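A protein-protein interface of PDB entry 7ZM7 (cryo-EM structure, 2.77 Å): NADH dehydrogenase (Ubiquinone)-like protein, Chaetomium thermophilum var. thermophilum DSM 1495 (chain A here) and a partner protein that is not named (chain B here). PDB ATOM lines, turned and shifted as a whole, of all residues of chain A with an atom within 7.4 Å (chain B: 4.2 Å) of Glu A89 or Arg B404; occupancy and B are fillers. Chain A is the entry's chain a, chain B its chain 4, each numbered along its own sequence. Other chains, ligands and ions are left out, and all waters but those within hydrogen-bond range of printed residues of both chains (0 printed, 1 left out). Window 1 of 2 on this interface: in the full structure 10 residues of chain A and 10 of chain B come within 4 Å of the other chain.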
ATOM      1  N   ARG A  75     -15.397  30.581  18.610  1.00  0.00           N
ATOM      2  CA  ARG A  75     -15.805  29.190  18.561  1.00  0.00           C
ATOM      3  C   ARG A  75     -17.252  29.024  18.132  1.00  0.00           C
ATOM      4  O   ARG A  75     -17.739  27.894  18.062  1.00  0.00           O
ATOM      5  CB  ARG A  75     -15.549  28.552  19.920  1.00  0.00           C
ATOM      6  CG  ARG A  75     -14.080  28.422  20.190  1.00  0.00           C
ATOM      7  CD  ARG A  75     -13.803  27.946  21.560  1.00  0.00           C
ATOM      8  NE  ARG A  75     -13.513  29.055  22.459  1.00  0.00           N
ATOM      9  CZ  ARG A  75     -14.052  29.196  23.662  1.00  0.00           C
ATOM     10  NH1 ARG A  75     -13.721  30.232  24.411  1.00  0.00           N
ATOM     11  NH2 ARG A  75     -14.915  28.304  24.114  1.00  0.00           N
ATOM     12  N   GLN A  76     -17.943  30.126  17.857  1.00  0.00           N
ATOM     13  CA  GLN A  76     -19.206  30.122  17.137  1.00  0.00           C
ATOM     14  C   GLN A  76     -19.041  29.671  15.696  1.00  0.00           C
ATOM     15  O   GLN A  76     -20.004  29.198  15.092  1.00  0.00           O
ATOM     16  CB  GLN A  76     -19.810  31.532  17.218  1.00  0.00           C
ATOM     17  CG  GLN A  76     -20.983  31.834  16.322  1.00  0.00           C
ATOM     18  CD  GLN A  76     -21.061  33.313  15.963  1.00  0.00           C
ATOM     19  OE1 GLN A  76     -20.411  34.149  16.582  1.00  0.00           O
ATOM     20  NE2 GLN A  76     -21.830  33.630  14.932  1.00  0.00           N
ATOM     21  N   ARG A  78     -16.799  27.315  14.754  1.00  0.00           N
ATOM     22  CA  ARG A  78     -16.368  25.937  14.696  1.00  0.00           C
ATOM     23  C   ARG A  78     -17.531  25.052  14.292  1.00  0.00           C
ATOM     24  O   ARG A  78     -18.669  25.503  14.141  1.00  0.00           O
ATOM     25  CB  ARG A  78     -15.804  25.490  16.037  1.00  0.00           C
ATOM     26  CG  ARG A  78     -14.735  26.388  16.560  1.00  0.00           C
ATOM     27  CD  ARG A  78     -13.944  25.704  17.605  1.00  0.00           C
ATOM     28  NE  ARG A  78     -12.754  26.469  17.893  1.00  0.00           N
ATOM     29  CZ  ARG A  78     -11.752  26.040  18.637  1.00  0.00           C
ATOM     30  NH1 ARG A  78     -10.699  26.818  18.826  1.00  0.00           N
ATOM     31  NH2 ARG A  78     -11.808  24.838  19.191  1.00  0.00           N
ATOM     32  N   TRP A  84     -15.845  17.154  19.818  1.00  0.00           N
ATOM     33  CA  TRP A  84     -15.348  18.056  20.840  1.00  0.00           C
ATOM     34  C   TRP A  84     -15.365  17.392  22.210  1.00  0.00           C
ATOM     35  O   TRP A  84     -16.361  16.790  22.617  1.00  0.00           O
ATOM     36  CB  TRP A  84     -16.190  19.324  20.880  1.00  0.00           C
ATOM     37  CG  TRP A  84     -16.265  20.064  19.615  1.00  0.00           C
ATOM     38  CD1 TRP A  84     -17.388  20.370  18.925  1.00  0.00           C
ATOM     39  CD2 TRP A  84     -15.178  20.627  18.888  1.00  0.00           C
ATOM     40  NE1 TRP A  84     -17.075  21.082  17.809  1.00  0.00           N
ATOM     41  CE2 TRP A  84     -15.720  21.257  17.763  1.00  0.00           C
ATOM     42  CE3 TRP A  84     -13.796  20.662  19.081  1.00  0.00           C
ATOM     43  CZ2 TRP A  84     -14.935  21.911  16.830  1.00  0.00           C
ATOM     44  CZ3 TRP A  84     -13.023  21.309  18.159  1.00  0.00           C
ATOM     45  CH2 TRP A  84     -13.593  21.926  17.047  1.00  0.00           C
ATOM     46  N   TRP A  85     -14.256  17.524  22.934  1.00  0.00           N
ATOM     47  CA  TRP A  85     -14.226  17.046  24.308  1.00  0.00           C
ATOM     48  C   TRP A  85     -15.260  17.773  25.146  1.00  0.00           C
ATOM     49  O   TRP A  85     -15.835  17.202  26.077  1.00  0.00           O
ATOM     50  CB  TRP A  85     -12.837  17.238  24.892  1.00  0.00           C
ATOM     51  CG  TRP A  85     -12.799  17.100  26.347  1.00  0.00           C
ATOM     52  CD1 TRP A  85     -12.664  15.952  27.051  1.00  0.00           C
ATOM     53  CD2 TRP A  85     -12.921  18.149  27.299  1.00  0.00           C
ATOM     54  NE1 TRP A  85     -12.679  16.216  28.389  1.00  0.00           N
ATOM     55  CE2 TRP A  85     -12.836  17.564  28.571  1.00  0.00           C
ATOM     56  CE3 TRP A  85     -13.088  19.530  27.199  1.00  0.00           C
ATOM     57  CZ2 TRP A  85     -12.918  18.305  29.734  1.00  0.00           C
ATOM     58  CZ3 TRP A  85     -13.168  20.265  28.349  1.00  0.00           C
ATOM     59  CH2 TRP A  85     -13.083  19.652  29.606  1.00  0.00           C
ATOM     60  N   ASP A  86     -15.501  19.034  24.827  1.00  0.00           N
ATOM     61  CA  ASP A  86     -16.580  19.824  25.398  1.00  0.00           C
ATOM     62  C   ASP A  86     -17.486  20.239  24.250  1.00  0.00           C
ATOM     63  O   ASP A  86     -17.200  21.195  23.532  1.00  0.00           O
ATOM     64  CB  ASP A  86     -16.051  21.027  26.158  1.00  0.00           C
ATOM     65  CG  ASP A  86     -17.142  21.769  26.862  1.00  0.00           C
ATOM     66  OD1 ASP A  86     -17.645  21.277  27.884  1.00  0.00           O
ATOM     67  OD2 ASP A  86     -17.501  22.859  26.400  1.00  0.00           O
ATOM     68  N   LYS A  87     -18.589  19.458  24.100  1.00  0.00           N
ATOM     69  CA  LYS A  87     -19.496  19.699  22.949  1.00  0.00           C
ATOM     70  C   LYS A  87     -20.183  21.053  23.082  1.00  0.00           C
ATOM     71  O   LYS A  87     -20.379  21.686  22.031  1.00  0.00           O
ATOM     72  CB  LYS A  87     -20.520  18.565  22.828  1.00  0.00           C
ATOM     73  CG  LYS A  87     -19.931  17.191  22.536  1.00  0.00           C
ATOM     74  CD  LYS A  87     -20.975  16.100  22.459  1.00  0.00           C
ATOM     75  CE  LYS A  87     -22.003  16.340  21.373  1.00  0.00           C
ATOM     76  NZ  LYS A  87     -21.384  16.353  20.027  1.00  0.00           N
ATOM     77  N   GLN A  88     -20.539  21.493  24.288  1.00  0.00           N
ATOM     78  CA  GLN A  88     -21.328  22.749  24.461  1.00  0.00           C
ATOM     79  C   GLN A  88     -20.532  23.969  23.995  1.00  0.00           C
ATOM     80  O   GLN A  88     -21.130  24.829  23.328  1.00  0.00           O
ATOM     81  CB  GLN A  88     -21.728  22.912  25.922  1.00  0.00           C
ATOM     82  CG  GLN A  88     -22.326  21.648  26.515  1.00  0.00           C
ATOM     83  CD  GLN A  88     -22.666  21.817  27.974  1.00  0.00           C
ATOM     84  OE1 GLN A  88     -22.981  20.857  28.668  1.00  0.00           O
ATOM     85  NE2 GLN A  88     -22.595  23.049  28.448  1.00  0.00           N
ATOM     86  N   GLU A  89     -19.250  24.053  24.351  1.00  0.00           N
ATOM     87  CA  GLU A  89     -18.411  25.181  23.981  1.00  0.00           C
ATOM     88  C   GLU A  89     -17.570  24.917  22.748  1.00  0.00           C
ATOM     89  O   GLU A  89     -16.905  25.839  22.270  1.00  0.00           O
ATOM     90  CB  GLU A  89     -17.491  25.554  25.143  1.00  0.00           C
ATOM     91  CG  GLU A  89     -18.174  26.104  26.382  1.00  0.00           C
ATOM     92  CD  GLU A  89     -18.815  27.469  26.161  1.00  0.00           C
ATOM     93  OE1 GLU A  89     -18.281  28.250  25.345  1.00  0.00           O
ATOM     94  OE2 GLU A  89     -19.839  27.772  26.811  1.00  0.00           O
ATOM     95  N   ARG A  90     -17.580  23.689  22.230  1.00  0.00           N
ATOM     96  CA  ARG A  90     -16.821  23.289  21.046  1.00  0.00           C
ATOM     97  C   ARG A  90     -15.317  23.456  21.267  1.00  0.00           C
ATOM     98  O   ARG A  90     -14.634  24.204  20.574  1.00  0.00           O
ATOM     99  CB  ARG A  90     -17.287  24.055  19.813  1.00  0.00           C
ATOM    100  CG  ARG A  90     -18.760  23.936  19.579  1.00  0.00           C
ATOM    101  CD  ARG A  90     -19.216  24.922  18.573  1.00  0.00           C
ATOM    102  NE  ARG A  90     -20.659  24.912  18.428  1.00  0.00           N
ATOM    103  CZ  ARG A  90     -21.317  25.732  17.624  1.00  0.00           C
ATOM    104  NH1 ARG A  90     -20.652  26.620  16.909  1.00  0.00           N
ATOM    105  NH2 ARG A  90     -22.631  25.662  17.537  1.00  0.00           N
ATOM    106  N   ARG A  91     -14.811  22.706  22.239  1.00  0.00           N
ATOM    107  CA  ARG A  91     -13.422  22.788  22.654  1.00  0.00           C
ATOM    108  C   ARG A  91     -12.890  21.378  22.869  1.00  0.00           C
ATOM    109  O   ARG A  91     -13.637  20.489  23.275  1.00  0.00           O
ATOM    110  CB  ARG A  91     -13.292  23.633  23.942  1.00  0.00           C
ATOM    111  CG  ARG A  91     -11.873  23.915  24.389  1.00  0.00           C
ATOM    112  CD  ARG A  91     -11.818  24.738  25.659  1.00  0.00           C
ATOM    113  NE  ARG A  91     -10.441  25.048  26.017  1.00  0.00           N
ATOM    114  CZ  ARG A  91      -9.676  24.289  26.787  1.00  0.00           C
ATOM    115  NH1 ARG A  91     -10.161  23.175  27.304  1.00  0.00           N
ATOM    116  NH2 ARG A  91      -8.428  24.648  27.046  1.00  0.00           N
ATOM    117  N   ASN A  92     -11.616  21.163  22.578  1.00  0.00           N
ATOM    118  CA  ASN A  92     -10.955  19.927  22.975  1.00  0.00           C
ATOM    119  C   ASN A  92     -10.077  20.199  24.180  1.00  0.00           C
ATOM    120  O   ASN A  92      -9.707  21.341  24.450  1.00  0.00           O
ATOM    121  CB  ASN A  92     -10.115  19.338  21.845  1.00  0.00           C
ATOM    122  CG  ASN A  92     -10.950  18.698  20.775  1.00  0.00           C
ATOM    123  OD1 ASN A  92     -11.977  18.088  21.051  1.00  0.00           O
ATOM    124  ND2 ASN A  92     -10.509  18.829  19.538  1.00  0.00           N
ATOM    125  N   GLU A  95      -6.347  21.931  23.929  1.00  0.00           N
ATOM    126  CA  GLU A  95      -6.155  22.845  22.774  1.00  0.00           C
ATOM    127  C   GLU A  95      -5.606  24.204  23.204  1.00  0.00           C
ATOM    128  O   GLU A  95      -6.031  24.686  24.269  1.00  0.00           O
ATOM    129  CB  GLU A  95      -7.455  22.973  21.974  1.00  0.00           C
ATOM    130  CG  GLU A  95      -8.453  23.959  22.545  1.00  0.00           C
ATOM    131  CD  GLU A  95      -9.646  24.194  21.635  1.00  0.00           C
ATOM    132  OE1 GLU A  95     -10.272  25.265  21.748  1.00  0.00           O
ATOM    133  OE2 GLU A  95      -9.946  23.301  20.821  1.00  0.00           O
ATOM    134  N   HIS A 101      -9.717  34.502  25.325  1.00  0.00           N
ATOM    135  CA  HIS A 101     -10.635  33.347  25.523  1.00  0.00           C
ATOM    136  C   HIS A 101     -11.963  33.769  26.162  1.00  0.00           C
ATOM    137  O   HIS A 101     -12.987  33.175  25.784  1.00  0.00           O
ATOM    138  CB  HIS A 101      -9.901  32.253  26.312  1.00  0.00           C
ATOM    139  CG  HIS A 101     -10.611  30.944  26.389  1.00  0.00           C
ATOM    140  ND1 HIS A 101     -10.519  29.999  25.393  1.00  0.00           N
ATOM    141  CD2 HIS A 101     -11.398  30.409  27.346  1.00  0.00           C
ATOM    142  CE1 HIS A 101     -11.222  28.937  25.730  1.00  0.00           C
ATOM    143  NE2 HIS A 101     -11.774  29.166  26.923  1.00  0.00           N
ATOM    144  N   LEU A 104     -14.362  34.917  23.320  1.00  0.00           N
ATOM    145  CA  LEU A 104     -14.364  34.169  22.077  1.00  0.00           C
ATOM    146  C   LEU A 104     -15.229  32.930  22.170  1.00  0.00           C
ATOM    147  O   LEU A 104     -15.363  32.205  21.181  1.00  0.00           O
ATOM    148  CB  LEU A 104     -12.948  33.757  21.699  1.00  0.00           C
ATOM    149  CG  LEU A 104     -11.966  34.751  21.094  1.00  0.00           C
ATOM    150  CD1 LEU A 104     -10.597  34.119  21.057  1.00  0.00           C
ATOM    151  CD2 LEU A 104     -12.380  35.145  19.718  1.00  0.00           C
ATOM    152  N   GLY A 105     -15.817  32.675  23.336  1.00  0.00           N
ATOM    153  CA  GLY A 105     -16.514  31.441  23.594  1.00  0.00           C
ATOM    154  C   GLY A 105     -17.929  31.449  23.100  1.00  0.00           C
ATOM    155  O   GLY A 105     -18.417  32.411  22.520  1.00  0.00           O
ATOM    156  N   MET A 106     -18.598  30.329  23.337  1.00  0.00           N
ATOM    157  CA  MET A 106     -19.978  30.197  22.899  1.00  0.00           C
ATOM    158  C   MET A 106     -20.910  31.086  23.698  1.00  0.00           C
ATOM    159  O   MET A 106     -21.998  31.416  23.226  1.00  0.00           O
ATOM    160  CB  MET A 106     -20.404  28.737  22.964  1.00  0.00           C
ATOM    161  CG  MET A 106     -19.888  27.936  21.777  1.00  0.00           C
ATOM    162  SD  MET A 106     -20.533  28.499  20.195  1.00  0.00           S
ATOM    163  CE  MET A 106     -22.228  28.862  20.603  1.00  0.00           C
ATOM    164  N   PHE A 107     -20.510  31.483  24.897  1.00  0.00           N
ATOM    165  CA  PHE A 107     -21.292  32.432  25.680  1.00  0.00           C
ATOM    166  C   PHE A 107     -20.602  33.792  25.675  1.00  0.00           C
ATOM    167  O   PHE A 107     -20.020  34.250  26.648  1.00  0.00           O
ATOM    168  CB  PHE A 107     -21.536  31.881  27.073  1.00  0.00           C
ATOM    169  CG  PHE A 107     -22.357  32.763  27.934  1.00  0.00           C
ATOM    170  CD1 PHE A 107     -23.427  33.468  27.404  1.00  0.00           C
ATOM    171  CD2 PHE A 107     -22.178  32.765  29.300  1.00  0.00           C
ATOM    172  CE1 PHE A 107     -24.213  34.248  28.194  1.00  0.00           C
ATOM    173  CE2 PHE A 107     -22.983  33.525  30.092  1.00  0.00           C
ATOM    174  CZ  PHE A 107     -24.004  34.272  29.528  1.00  0.00           C
ATOM    175  N   SER A 108     -20.707  34.434  24.523  1.00  0.00           N
ATOM    176  CA  SER A 108     -20.036  35.690  24.237  1.00  0.00           C
ATOM    177  C   SER A 108     -20.824  36.392  23.143  1.00  0.00           C
ATOM    178  O   SER A 108     -21.655  35.763  22.484  1.00  0.00           O
ATOM    179  CB  SER A 108     -18.576  35.455  23.810  1.00  0.00           C
ATOM    180  OG  SER A 108     -18.482  34.930  22.504  1.00  0.00           O
ATOM    181  N   PHE B 403     -15.397  26.936  35.602  1.00  0.00           N
ATOM    182  CA  PHE B 403     -16.687  26.887  36.263  1.00  0.00           C
ATOM    183  C   PHE B 403     -17.788  27.011  35.229  1.00  0.00           C
ATOM    184  O   PHE B 403     -17.603  27.654  34.195  1.00  0.00           O
ATOM    185  CB  PHE B 403     -16.806  27.994  37.297  1.00  0.00           C
ATOM    186  CG  PHE B 403     -15.785  27.908  38.386  1.00  0.00           C
ATOM    187  CD1 PHE B 403     -15.982  27.080  39.466  1.00  0.00           C
ATOM    188  CD2 PHE B 403     -14.635  28.661  38.334  1.00  0.00           C
ATOM    189  CE1 PHE B 403     -15.057  27.002  40.450  1.00  0.00           C
ATOM    190  CE2 PHE B 403     -13.702  28.584  39.319  1.00  0.00           C
ATOM    191  CZ  PHE B 403     -13.913  27.758  40.378  1.00  0.00           C
ATOM    192  N   ARG B 404     -18.915  26.361  35.494  1.00  0.00           N
ATOM    193  CA  ARG B 404     -20.064  26.425  34.609  1.00  0.00           C
ATOM    194  C   ARG B 404     -21.209  25.647  35.234  1.00  0.00           C
ATOM    195  O   ARG B 404     -21.007  24.541  35.732  1.00  0.00           O
ATOM    196  CB  ARG B 404     -19.726  25.846  33.233  1.00  0.00           C
ATOM    197  CG  ARG B 404     -20.643  26.280  32.136  1.00  0.00           C
ATOM    198  CD  ARG B 404     -20.323  25.582  30.843  1.00  0.00           C
ATOM    199  NE  ARG B 404     -20.139  24.147  31.025  1.00  0.00           N
ATOM    200  CZ  ARG B 404     -19.488  23.355  30.178  1.00  0.00           C
ATOM    201  NH1 ARG B 404     -18.964  23.845  29.076  1.00  0.00           N
ATOM    202  NH2 ARG B 404     -19.372  22.066  30.431  1.00  0.00           N
ATOM    203  N   GLY B 405     -22.401  26.225  35.196  1.00  0.00           N
ATOM    204  CA  GLY B 405     -23.584  25.472  35.552  1.00  0.00           C
ATOM    205  C   GLY B 405     -23.562  24.875  36.938  1.00  0.00           C
ATOM    206  O   GLY B 405     -24.029  23.750  37.134  1.00  0.00           O
ATOM    207  N   LEU B 406     -23.055  25.614  37.913  1.00  0.00           N
ATOM    208  CA  LEU B 406     -23.012  25.137  39.281  1.00  0.00           C
ATOM    209  C   LEU B 406     -24.384  25.088  39.932  1.00  0.00           C
ATOM    210  O   LEU B 406     -24.483  24.656  41.080  1.00  0.00           O
ATOM    211  CB  LEU B 406     -22.082  26.021  40.096  1.00  0.00           C
ATOM    212  CG  LEU B 406     -20.630  25.629  39.879  1.00  0.00           C
ATOM    213  CD1 LEU B 406     -19.696  26.553  40.615  1.00  0.00           C
ATOM    214  CD2 LEU B 406     -20.420  24.188  40.282  1.00  0.00           C
ATOM    215  N   ARG B 471     -21.995  33.047  34.189  1.00  0.00           N
ATOM    216  CA  ARG B 471     -20.868  32.170  33.814  1.00  0.00           C
ATOM    217  C   ARG B 471     -20.666  31.039  34.828  1.00  0.00           C
ATOM    218  O   ARG B 471     -20.294  29.941  34.399  1.00  0.00           O
ATOM    219  CB  ARG B 471     -19.607  33.006  33.595  1.00  0.00           C
ATOM    220  CG  ARG B 471     -19.493  33.609  32.203  1.00  0.00           C
ATOM    221  CD  ARG B 471     -18.241  34.453  32.111  1.00  0.00           C
ATOM    222  NE  ARG B 471     -18.315  35.621  32.972  1.00  0.00           N
ATOM    223  CZ  ARG B 471     -17.312  36.462  33.180  1.00  0.00           C
ATOM    224  NH1 ARG B 471     -17.472  37.501  33.979  1.00  0.00           N
ATOM    225  NH2 ARG B 471     -16.147  36.254  32.595  1.00  0.00           N
ATOM    226  N   ILE B 472     -20.843  31.295  36.125  1.00  0.00           N
ATOM    227  CA  ILE B 472     -20.522  30.257  37.150  1.00  0.00           C
ATOM    228  C   ILE B 472     -21.724  29.374  37.478  1.00  0.00           C
ATOM    229  O   ILE B 472     -21.572  28.155  37.408  1.00  0.00           O
ATOM    230  CB  ILE B 472     -19.913  30.929  38.400  1.00  0.00           C
ATOM    231  CG1 ILE B 472     -18.699  31.791  38.054  1.00  0.00           C
ATOM    232  CG2 ILE B 472     -19.593  29.910  39.480  1.00  0.00           C
ATOM    233  CD1 ILE B 472     -18.047  32.424  39.252  1.00  0.00           C
ATOM    234  N   PHE B 474     -24.985  29.504  36.038  1.00  0.00           N
ATOM    235  CA  PHE B 474     -25.679  29.158  34.815  1.00  0.00           C
ATOM    236  C   PHE B 474     -24.612  29.026  33.741  1.00  0.00           C
ATOM    237  O   PHE B 474     -23.422  28.931  34.032  1.00  0.00           O
ATOM    238  CB  PHE B 474     -26.702  30.226  34.419  1.00  0.00           C
ATOM    239  CG  PHE B 474     -27.839  30.418  35.384  1.00  0.00           C
ATOM    240  CD1 PHE B 474     -28.068  29.545  36.424  1.00  0.00           C
ATOM    241  CD2 PHE B 474     -28.684  31.496  35.238  1.00  0.00           C
ATOM    242  CE1 PHE B 474     -29.107  29.739  37.289  1.00  0.00           C
ATOM    243  CE2 PHE B 474     -29.725  31.688  36.103  1.00  0.00           C
ATOM    244  CZ  PHE B 474     -29.941  30.804  37.127  1.00  0.00           C
ATOM    245  N   GLY B 475     -25.032  29.025  32.490  1.00  0.00           N
ATOM    246  CA  GLY B 475     -24.104  29.167  31.395  1.00  0.00           C
ATOM    247  C   GLY B 475     -23.689  27.886  30.731  1.00  0.00           C
ATOM    248  O   GLY B 475     -22.593  27.830  30.174  1.00  0.00           O
ATOM    249  N   GLY B 476     -24.534  26.869  30.751  1.00  0.00           N
ATOM    250  CA  GLY B 476     -24.188  25.570  30.236  1.00  0.00           C
ATOM    251  C   GLY B 476     -24.604  24.529  31.236  1.00  0.00           C
ATOM    252  O   GLY B 476     -25.603  24.702  31.927  1.00  0.00           O
ATOM    253  N   SER B 477     -23.859  23.448  31.318  1.00  0.00           N
ATOM    254  CA  SER B 477     -24.090  22.390  32.280  1.00  0.00           C
ATOM    255  C   SER B 477     -22.914  22.340  33.226  1.00  0.00           C
ATOM    256  O   SER B 477     -21.917  23.031  33.028  1.00  0.00           O
ATOM    257  CB  SER B 477     -24.283  21.059  31.566  1.00  0.00           C
ATOM    258  OG  SER B 477     -25.529  21.031  30.923  1.00  0.00           O
ATOM    259  N   VAL B 478     -23.030  21.507  34.258  1.00  0.00           N
ATOM    260  CA  VAL B 478     -21.894  21.297  35.141  1.00  0.00           C
ATOM    261  C   VAL B 478     -20.657  21.057  34.292  1.00  0.00           C
ATOM    262  O   VAL B 478     -20.666  20.237  33.371  1.00  0.00           O
ATOM    263  CB  VAL B 478     -22.163  20.137  36.112  1.00  0.00           C
ATOM    264  CG1 VAL B 478     -20.900  19.787  36.837  1.00  0.00           C
ATOM    265  CG2 VAL B 478     -23.215  20.533  37.097  1.00  0.00           C
ATOM    266  N   SER B 479     -19.605  21.813  34.575  1.00  0.00           N
ATOM    267  CA  SER B 479     -18.443  21.855  33.708  1.00  0.00           C
ATOM    268  C   SER B 479     -17.748  20.506  33.659  1.00  0.00           C
ATOM    269  O   SER B 479     -17.804  19.711  34.597  1.00  0.00           O
ATOM    270  CB  SER B 479     -17.474  22.933  34.184  1.00  0.00           C
ATOM    271  OG  SER B 479     -16.713  22.486  35.283  1.00  0.00           O
ATOM    272  N   LEU B 480     -17.086  20.250  32.546  1.00  0.00           N
ATOM    273  CA  LEU B 480     -16.402  18.986  32.357  1.00  0.00           C
ATOM    274  C   LEU B 480     -15.040  18.937  33.018  1.00  0.00           C
ATOM    275  O   LEU B 480     -14.445  17.860  33.081  1.00  0.00           O
ATOM    276  CB  LEU B 480     -16.267  18.692  30.869  1.00  0.00           C
ATOM    277  CG  LEU B 480     -17.583  18.726  30.105  1.00  0.00           C
ATOM    278  CD1 LEU B 480     -17.339  18.330  28.680  1.00  0.00           C
ATOM    279  CD2 LEU B 480     -18.600  17.812  30.746  1.00  0.00           C
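OD1 of Asp A86 is in salt-bridge range of NH1 of Arg B404 (3.1 Å). N of Ser B477 sits close to NE2 of Gln A88 (3.2 Å).
OE1 of Glu A89 lies within salt-bridge range of NH2 of Arg A75 (3.6 Å). The backbone NH (N) of Trp A85 is in hydrogen-bond range of the backbone carbonyl oxygen (O) of Arg A91 (3.0 Å). The side-chain amide oxygen (OD1) of Asn A92 lies within hydrogen-bond range of the backbone NH (N) of Trp A85. The backbone carbonyl oxygen (O) of Arg A91 sits at hydrogen-bond distance from the backbone NH (N) of Asp A86, 2.8 Å away. N of Met A106 sits at hydrogen-bond distance from OE1 of Glu A89, at 2.9 Å. The backbone carbonyl oxygen (O) of Arg B404 is in hydrogen-bond range of the backbone NH (N) of Ser B479 (3.3 Å).
Among the printed residues, merely in contact across the chains: Asp A86 with Leu B480, Trp A85 with Leu B480, Gln A88 with Gly B476, Gln A88 with Arg B404 and Glu A89 with Arg B404.
Glu A89 touches one residue of chain B. Arg B404 touches just these residues of chain A: Asp A86 (3.1 Å), Gln A88 (3.6 Å) and Glu A89 (3.6 Å). Printed residues of chain A within 4 Å of Gly B476: Gln A88. Of the printed residues of chain A, Leu B480 touches Trp A85 and Asp A86. Of the printed residues of chain B, Asp A86 touches Arg B404 and Leu B480. Printed residues of chain B within 4 Å of Gln A88: Arg B404 (3.6 Å), Gly B476 (3.5 Å) and Ser B477 (3.2 Å). Lys A87 touches none of the printed residues of chain B. The nearest printed residue of chain B that does not touch Glu A89 is Gly B475 (4.3 Å). The nearest residue of chain A that does not touch Arg B404 is Lys A87 (6.6 Å). The nearest printed residue of chain B that does not touch Gln A88 is Gly B475 (5.1 Å).
Hydrophobic or aromatic side chains of chain A that line the printed part of chain B: Trp A85. Along chain A the printed residues that touch a printed residue of chain B span positions 85 to 89. Of the 13 printed residues of chain B, 4 touch a printed residue of chain A. Hydrophobic or aromatic side chains of chain B that line the printed part of chain A: Leu B480. Among the printed residues, 7 pairs touch across the chains.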
